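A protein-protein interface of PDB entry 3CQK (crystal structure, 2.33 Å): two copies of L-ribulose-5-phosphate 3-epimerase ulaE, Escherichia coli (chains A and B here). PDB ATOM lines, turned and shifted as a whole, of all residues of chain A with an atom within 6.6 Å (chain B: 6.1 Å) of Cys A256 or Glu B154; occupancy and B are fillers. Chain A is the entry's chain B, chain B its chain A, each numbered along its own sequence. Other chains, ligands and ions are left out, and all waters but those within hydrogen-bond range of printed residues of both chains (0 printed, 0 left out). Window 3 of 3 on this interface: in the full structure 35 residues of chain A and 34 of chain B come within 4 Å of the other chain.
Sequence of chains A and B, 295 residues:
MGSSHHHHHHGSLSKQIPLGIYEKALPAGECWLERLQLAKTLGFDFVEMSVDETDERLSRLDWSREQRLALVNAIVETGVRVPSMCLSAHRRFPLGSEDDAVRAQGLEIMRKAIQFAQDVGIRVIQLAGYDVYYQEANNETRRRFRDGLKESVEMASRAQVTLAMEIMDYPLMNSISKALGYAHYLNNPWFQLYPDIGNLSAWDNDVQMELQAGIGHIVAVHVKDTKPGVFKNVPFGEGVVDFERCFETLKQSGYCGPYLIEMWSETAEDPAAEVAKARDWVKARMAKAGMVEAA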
ATOM      1  N   GLN A  16      -7.364   2.796  31.143  1.00  0.00           N
ATOM      2  CA  GLN A  16      -8.146   1.914  32.067  1.00  0.00           C
ATOM      3  C   GLN A  16      -7.236   0.916  32.767  1.00  0.00           C
ATOM      4  O   GLN A  16      -6.351   0.321  32.139  1.00  0.00           O
ATOM      5  CB  GLN A  16      -9.233   1.147  31.309  1.00  0.00           C
ATOM      6  CG  GLN A  16     -10.094   1.996  30.369  1.00  0.00           C
ATOM      7  CD  GLN A  16     -11.174   1.181  29.659  1.00  0.00           C
ATOM      8  OE1 GLN A  16     -10.890   0.160  29.010  1.00  0.00           O
ATOM      9  NE2 GLN A  16     -12.424   1.639  29.772  1.00  0.00           N
ATOM     10  N   ILE A  17      -7.429   0.781  34.076  1.00  0.00           N
ATOM     11  CA  ILE A  17      -6.948  -0.369  34.841  1.00  0.00           C
ATOM     12  C   ILE A  17      -8.230  -1.073  35.297  1.00  0.00           C
ATOM     13  O   ILE A  17      -8.974  -0.516  36.098  1.00  0.00           O
ATOM     14  CB  ILE A  17      -6.117   0.060  36.080  1.00  0.00           C
ATOM     15  CG1 ILE A  17      -4.842   0.807  35.660  1.00  0.00           C
ATOM     16  CG2 ILE A  17      -5.762  -1.149  36.952  1.00  0.00           C
ATOM     17  CD1 ILE A  17      -4.344   1.804  36.690  1.00  0.00           C
ATOM     18  N   PRO A  18      -8.521  -2.279  34.764  1.00  0.00           N
ATOM     19  CA  PRO A  18      -9.732  -2.960  35.234  1.00  0.00           C
ATOM     20  C   PRO A  18      -9.566  -3.400  36.685  1.00  0.00           C
ATOM     21  O   PRO A  18      -8.628  -4.124  37.000  1.00  0.00           O
ATOM     22  CB  PRO A  18      -9.854  -4.173  34.300  1.00  0.00           C
ATOM     23  CG  PRO A  18      -8.873  -3.954  33.216  1.00  0.00           C
ATOM     24  CD  PRO A  18      -7.804  -3.075  33.753  1.00  0.00           C
ATOM     25  N   ILE A 215       6.458 -11.772  33.156  1.00  0.00           N
ATOM     26  CA  ILE A 215       5.636 -10.732  32.545  1.00  0.00           C
ATOM     27  C   ILE A 215       4.833 -11.127  31.280  1.00  0.00           C
ATOM     28  O   ILE A 215       3.619 -10.852  31.208  1.00  0.00           O
ATOM     29  CB  ILE A 215       6.403  -9.374  32.435  1.00  0.00           C
ATOM     30  CG1 ILE A 215       5.626  -8.259  33.158  1.00  0.00           C
ATOM     31  CG2 ILE A 215       6.821  -9.042  31.001  1.00  0.00           C
ATOM     32  CD1 ILE A 215       4.240  -7.948  32.619  1.00  0.00           C
ATOM     33  N   LEU A 250       5.119  -3.773  37.768  1.00  0.00           N
ATOM     34  CA  LEU A 250       4.151  -4.194  36.761  1.00  0.00           C
ATOM     35  C   LEU A 250       3.865  -3.090  35.722  1.00  0.00           C
ATOM     36  O   LEU A 250       3.888  -3.350  34.526  1.00  0.00           O
ATOM     37  CB  LEU A 250       2.880  -4.737  37.429  1.00  0.00           C
ATOM     38  CG  LEU A 250       3.062  -6.077  38.174  1.00  0.00           C
ATOM     39  CD1 LEU A 250       1.977  -6.288  39.201  1.00  0.00           C
ATOM     40  CD2 LEU A 250       3.147  -7.290  37.234  1.00  0.00           C
ATOM     41  N   GLY A 254       5.197  -3.386  31.479  1.00  0.00           N
ATOM     42  CA  GLY A 254       4.244  -3.512  30.373  1.00  0.00           C
ATOM     43  C   GLY A 254       2.989  -4.330  30.664  1.00  0.00           C
ATOM     44  O   GLY A 254       2.313  -4.789  29.745  1.00  0.00           O
ATOM     45  N   TYR A 255       2.669  -4.507  31.941  1.00  0.00           N
ATOM     46  CA  TYR A 255       1.439  -5.197  32.333  1.00  0.00           C
ATOM     47  C   TYR A 255       0.229  -4.309  32.117  1.00  0.00           C
ATOM     48  O   TYR A 255       0.160  -3.206  32.653  1.00  0.00           O
ATOM     49  CB  TYR A 255       1.491  -5.656  33.794  1.00  0.00           C
ATOM     50  CG  TYR A 255       0.254  -6.398  34.189  1.00  0.00           C
ATOM     51  CD1 TYR A 255      -0.095  -7.581  33.539  1.00  0.00           C
ATOM     52  CD2 TYR A 255      -0.583  -5.912  35.189  1.00  0.00           C
ATOM     53  CE1 TYR A 255      -1.233  -8.257  33.864  1.00  0.00           C
ATOM     54  CE2 TYR A 255      -1.742  -6.591  35.537  1.00  0.00           C
ATOM     55  CZ  TYR A 255      -2.053  -7.770  34.866  1.00  0.00           C
ATOM     56  OH  TYR A 255      -3.173  -8.470  35.182  1.00  0.00           O
ATOM     57  N   CYS A 256      -0.724  -4.797  31.328  1.00  0.00           N
ATOM     58  CA  CYS A 256      -1.930  -4.027  31.031  1.00  0.00           C
ATOM     59  C   CYS A 256      -3.227  -4.685  31.451  1.00  0.00           C
ATOM     60  O   CYS A 256      -4.299  -4.264  31.004  1.00  0.00           O
ATOM     61  CB  CYS A 256      -2.005  -3.712  29.534  1.00  0.00           C
ATOM     62  SG  CYS A 256      -0.938  -2.356  29.105  1.00  0.00           S
ATOM     63  N   GLY A 257      -3.135  -5.688  32.319  1.00  0.00           N
ATOM     64  CA  GLY A 257      -4.274  -6.513  32.667  1.00  0.00           C
ATOM     65  C   GLY A 257      -5.004  -6.052  33.906  1.00  0.00           C
ATOM     66  O   GLY A 257      -4.650  -5.039  34.501  1.00  0.00           O
ATOM     67  N   PRO A 258      -6.037  -6.807  34.303  1.00  0.00           N
ATOM     68  CA  PRO A 258      -6.822  -6.527  35.515  1.00  0.00           C
ATOM     69  C   PRO A 258      -6.103  -6.797  36.843  1.00  0.00           C
ATOM     70  O   PRO A 258      -5.145  -7.586  36.899  1.00  0.00           O
ATOM     71  CB  PRO A 258      -8.002  -7.492  35.381  1.00  0.00           C
ATOM     72  CG  PRO A 258      -7.468  -8.634  34.553  1.00  0.00           C
ATOM     73  CD  PRO A 258      -6.537  -7.992  33.575  1.00  0.00           C
ATOM     74  N   TYR A 259      -6.595  -6.147  37.900  1.00  0.00           N
ATOM     75  CA  TYR A 259      -6.199  -6.445  39.283  1.00  0.00           C
ATOM     76  C   TYR A 259      -7.442  -6.814  40.076  1.00  0.00           C
ATOM     77  O   TYR A 259      -8.450  -6.117  40.015  1.00  0.00           O
ATOM     78  CB  TYR A 259      -5.536  -5.237  39.940  1.00  0.00           C
ATOM     79  CG  TYR A 259      -4.213  -4.844  39.355  1.00  0.00           C
ATOM     80  CD1 TYR A 259      -3.025  -5.226  39.968  1.00  0.00           C
ATOM     81  CD2 TYR A 259      -4.142  -4.079  38.193  1.00  0.00           C
ATOM     82  CE1 TYR A 259      -1.811  -4.867  39.445  1.00  0.00           C
ATOM     83  CE2 TYR A 259      -2.913  -3.710  37.652  1.00  0.00           C
ATOM     84  CZ  TYR A 259      -1.756  -4.108  38.286  1.00  0.00           C
ATOM     85  OH  TYR A 259      -0.529  -3.744  37.771  1.00  0.00           O
ATOM     86  N   LEU B 149      -1.353  -2.562  16.674  1.00  0.00           N
ATOM     87  CA  LEU B 149      -1.334  -3.912  17.168  1.00  0.00           C
ATOM     88  C   LEU B 149      -1.102  -3.914  18.671  1.00  0.00           C
ATOM     89  O   LEU B 149      -1.798  -4.614  19.402  1.00  0.00           O
ATOM     90  CB  LEU B 149      -0.239  -4.687  16.449  1.00  0.00           C
ATOM     91  CG  LEU B 149      -0.467  -6.163  16.199  1.00  0.00           C
ATOM     92  CD1 LEU B 149      -1.882  -6.422  15.671  1.00  0.00           C
ATOM     93  CD2 LEU B 149       0.575  -6.634  15.206  1.00  0.00           C
ATOM     94  N   LYS B 150      -0.136  -3.107  19.119  1.00  0.00           N
ATOM     95  CA  LYS B 150       0.173  -2.913  20.541  1.00  0.00           C
ATOM     96  C   LYS B 150      -1.050  -2.409  21.276  1.00  0.00           C
ATOM     97  O   LYS B 150      -1.389  -2.914  22.341  1.00  0.00           O
ATOM     98  CB  LYS B 150       1.369  -1.949  20.732  1.00  0.00           C
ATOM     99  CG  LYS B 150       1.891  -1.859  22.179  1.00  0.00           C
ATOM    100  CD  LYS B 150       3.420  -1.750  22.241  1.00  0.00           C
ATOM    101  CE  LYS B 150       3.988  -2.378  23.550  1.00  0.00           C
ATOM    102  NZ  LYS B 150       5.309  -3.121  23.389  1.00  0.00           N
ATOM    103  N   GLU B 151      -1.727  -1.438  20.675  1.00  0.00           N
ATOM    104  CA  GLU B 151      -2.925  -0.837  21.245  1.00  0.00           C
ATOM    105  C   GLU B 151      -4.121  -1.791  21.329  1.00  0.00           C
ATOM    106  O   GLU B 151      -4.876  -1.759  22.307  1.00  0.00           O
ATOM    107  CB  GLU B 151      -3.302   0.398  20.448  1.00  0.00           C
ATOM    108  CG  GLU B 151      -4.324   1.300  21.134  1.00  0.00           C
ATOM    109  CD  GLU B 151      -4.503   2.620  20.409  1.00  0.00           C
ATOM    110  OE1 GLU B 151      -3.649   2.956  19.549  1.00  0.00           O
ATOM    111  OE2 GLU B 151      -5.498   3.317  20.702  1.00  0.00           O
ATOM    112  N   SER B 152      -4.285  -2.623  20.301  1.00  0.00           N
ATOM    113  CA  SER B 152      -5.305  -3.662  20.265  1.00  0.00           C
ATOM    114  C   SER B 152      -5.051  -4.723  21.329  1.00  0.00           C
ATOM    115  O   SER B 152      -5.981  -5.182  21.995  1.00  0.00           O
ATOM    116  CB  SER B 152      -5.312  -4.338  18.898  1.00  0.00           C
ATOM    117  OG  SER B 152      -5.488  -3.398  17.858  1.00  0.00           O
ATOM    118  N   VAL B 153      -3.785  -5.105  21.469  1.00  0.00           N
ATOM    119  CA  VAL B 153      -3.355  -6.128  22.417  1.00  0.00           C
ATOM    120  C   VAL B 153      -3.474  -5.652  23.866  1.00  0.00           C
ATOM    121  O   VAL B 153      -3.776  -6.446  24.759  1.00  0.00           O
ATOM    122  CB  VAL B 153      -1.931  -6.652  22.071  1.00  0.00           C
ATOM    123  CG1 VAL B 153      -1.279  -7.289  23.259  1.00  0.00           C
ATOM    124  CG2 VAL B 153      -2.019  -7.640  20.930  1.00  0.00           C
ATOM    125  N   GLU B 154      -3.247  -4.363  24.086  1.00  0.00           N
ATOM    126  CA  GLU B 154      -3.520  -3.730  25.377  1.00  0.00           C
ATOM    127  C   GLU B 154      -5.003  -3.812  25.777  1.00  0.00           C
ATOM    128  O   GLU B 154      -5.317  -4.173  26.910  1.00  0.00           O
ATOM    129  CB  GLU B 154      -3.023  -2.290  25.382  1.00  0.00           C
ATOM    130  CG  GLU B 154      -1.482  -2.197  25.456  1.00  0.00           C
ATOM    131  CD  GLU B 154      -0.958  -0.769  25.406  1.00  0.00           C
ATOM    132  OE1 GLU B 154      -1.776   0.172  25.537  1.00  0.00           O
ATOM    133  OE2 GLU B 154       0.273  -0.589  25.234  1.00  0.00           O
ATOM    134  N   MET B 155      -5.894  -3.498  24.837  1.00  0.00           N
ATOM    135  CA  MET B 155      -7.334  -3.601  25.043  1.00  0.00           C
ATOM    136  C   MET B 155      -7.713  -5.030  25.363  1.00  0.00           C
ATOM    137  O   MET B 155      -8.545  -5.273  26.234  1.00  0.00           O
ATOM    138  CB  MET B 155      -8.088  -3.197  23.790  1.00  0.00           C
ATOM    139  CG  MET B 155      -8.107  -1.732  23.493  1.00  0.00           C
ATOM    140  SD  MET B 155      -8.974  -1.403  21.926  1.00  0.00           S
ATOM    141  CE  MET B 155      -9.317   0.335  22.223  1.00  0.00           C
ATOM    142  N   ALA B 156      -7.096  -5.960  24.628  1.00  0.00           N
ATOM    143  CA  ALA B 156      -7.289  -7.402  24.766  1.00  0.00           C
ATOM    144  C   ALA B 156      -6.810  -7.963  26.111  1.00  0.00           C
ATOM    145  O   ALA B 156      -7.394  -8.922  26.617  1.00  0.00           O
ATOM    146  CB  ALA B 156      -6.593  -8.113  23.627  1.00  0.00           C
ATOM    147  N   SER B 157      -5.740  -7.380  26.664  1.00  0.00           N
ATOM    148  CA  SER B 157      -5.230  -7.703  28.004  1.00  0.00           C
ATOM    149  C   SER B 157      -6.182  -7.310  29.100  1.00  0.00           C
ATOM    150  O   SER B 157      -6.319  -8.027  30.091  1.00  0.00           O
ATOM    151  CB  SER B 157      -3.914  -6.988  28.290  1.00  0.00           C
ATOM    152  OG  SER B 157      -2.971  -7.272  27.292  1.00  0.00           O
ATOM    153  N   ARG B 158      -6.798  -6.144  28.934  1.00  0.00           N
ATOM    154  CA  ARG B 158      -7.775  -5.636  29.886  1.00  0.00           C
ATOM    155  C   ARG B 158      -9.043  -6.500  29.904  1.00  0.00           C
ATOM    156  O   ARG B 158      -9.596  -6.774  30.965  1.00  0.00           O
ATOM    157  CB  ARG B 158      -8.112  -4.177  29.569  1.00  0.00           C
ATOM    158  CG  ARG B 158      -6.921  -3.252  29.794  1.00  0.00           C
ATOM    159  CD  ARG B 158      -7.323  -1.807  29.930  1.00  0.00           C
ATOM    160  NE  ARG B 158      -7.637  -1.206  28.641  1.00  0.00           N
ATOM    161  CZ  ARG B 158      -6.750  -0.589  27.865  1.00  0.00           C
ATOM    162  NH1 ARG B 158      -5.481  -0.487  28.249  1.00  0.00           N
ATOM    163  NH2 ARG B 158      -7.134  -0.080  26.698  1.00  0.00           N
ATOM    164  N   ALA B 159      -9.462  -6.945  28.726  1.00  0.00           N
ATOM    165  CA  ALA B 159     -10.677  -7.743  28.566  1.00  0.00           C
ATOM    166  C   ALA B 159     -10.411  -9.234  28.774  1.00  0.00           C
ATOM    167  O   ALA B 159     -11.347 -10.012  28.962  1.00  0.00           O
ATOM    168  CB  ALA B 159     -11.287  -7.507  27.163  1.00  0.00           C
ATOM    169  N   ASN B 188       3.014 -10.694  25.063  1.00  0.00           N
ATOM    170  CA  ASN B 188       1.744 -10.590  25.772  1.00  0.00           C
ATOM    171  C   ASN B 188       0.990 -11.906  25.591  1.00  0.00           C
ATOM    172  O   ASN B 188       0.869 -12.380  24.463  1.00  0.00           O
ATOM    173  CB  ASN B 188       0.923  -9.394  25.241  1.00  0.00           C
ATOM    174  CG  ASN B 188      -0.393  -9.168  26.028  1.00  0.00           C
ATOM    175  OD1 ASN B 188      -1.306  -9.992  25.996  1.00  0.00           O
ATOM    176  ND2 ASN B 188      -0.474  -8.060  26.740  1.00  0.00           N
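Arg B158 touches Gln A16 (CD to O, 3.2 Å). Pro A18 touches Arg B158. Cys A256 touches Glu B154 (SG to CG, 3.7 Å). Cys A256 touches Ser B157 (O to CB, 3.9 Å). Cys A256 touches Arg B158. CA of Gly A257 touches O of Ser B157, 3.6 Å away. Ser B157 touches Pro A258 (O to CD, 3.5 Å).
O of Pro A258 sits at hydrogen-bond distance from OH of Tyr A255, 2.8 Å away. The side-chain hydroxyl (OG) of Ser B157 is in hydrogen-bond range of the backbone carbonyl oxygen (O) of Val B153 (2.8 Å). The side-chain amide nitrogen (ND2) of Asn B188 lies within hydrogen-bond range of the side-chain hydroxyl (OG) of Ser B157 (2.7 Å). The backbone carbonyl oxygen (O) of Pro A18 is in hydrogen-bond range of the backbone NH (N) of Tyr A259, at 3.0 Å.
No position is printed for both chains.
Of the 11 printed residues of chain A, 5 touch a printed residue of chain B. Hydrophobic or aromatic side chains of chain A within 4 Å of the printed part of chain B: Pro A18 and Pro A258. Among the printed residues, no Asp or Glu carboxylate lies within 4 Å of a Lys or Arg side-chain nitrogen of the other chain.
Cys A256 touches three residues of chain B. Glu B154 touches one residue of chain A. Of the printed residues of chain B, Pro A18 touches Arg B158. Of the printed residues of chain A, Arg B158 touches Gln A16, Pro A18 and Cys A256. Leu A250 touches none of the printed residues of chain B. Ile A17 touches none of the printed residues of chain B. The nearest residue of chain A that does not touch Glu B154 is Gly A257 (6.0 Å).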
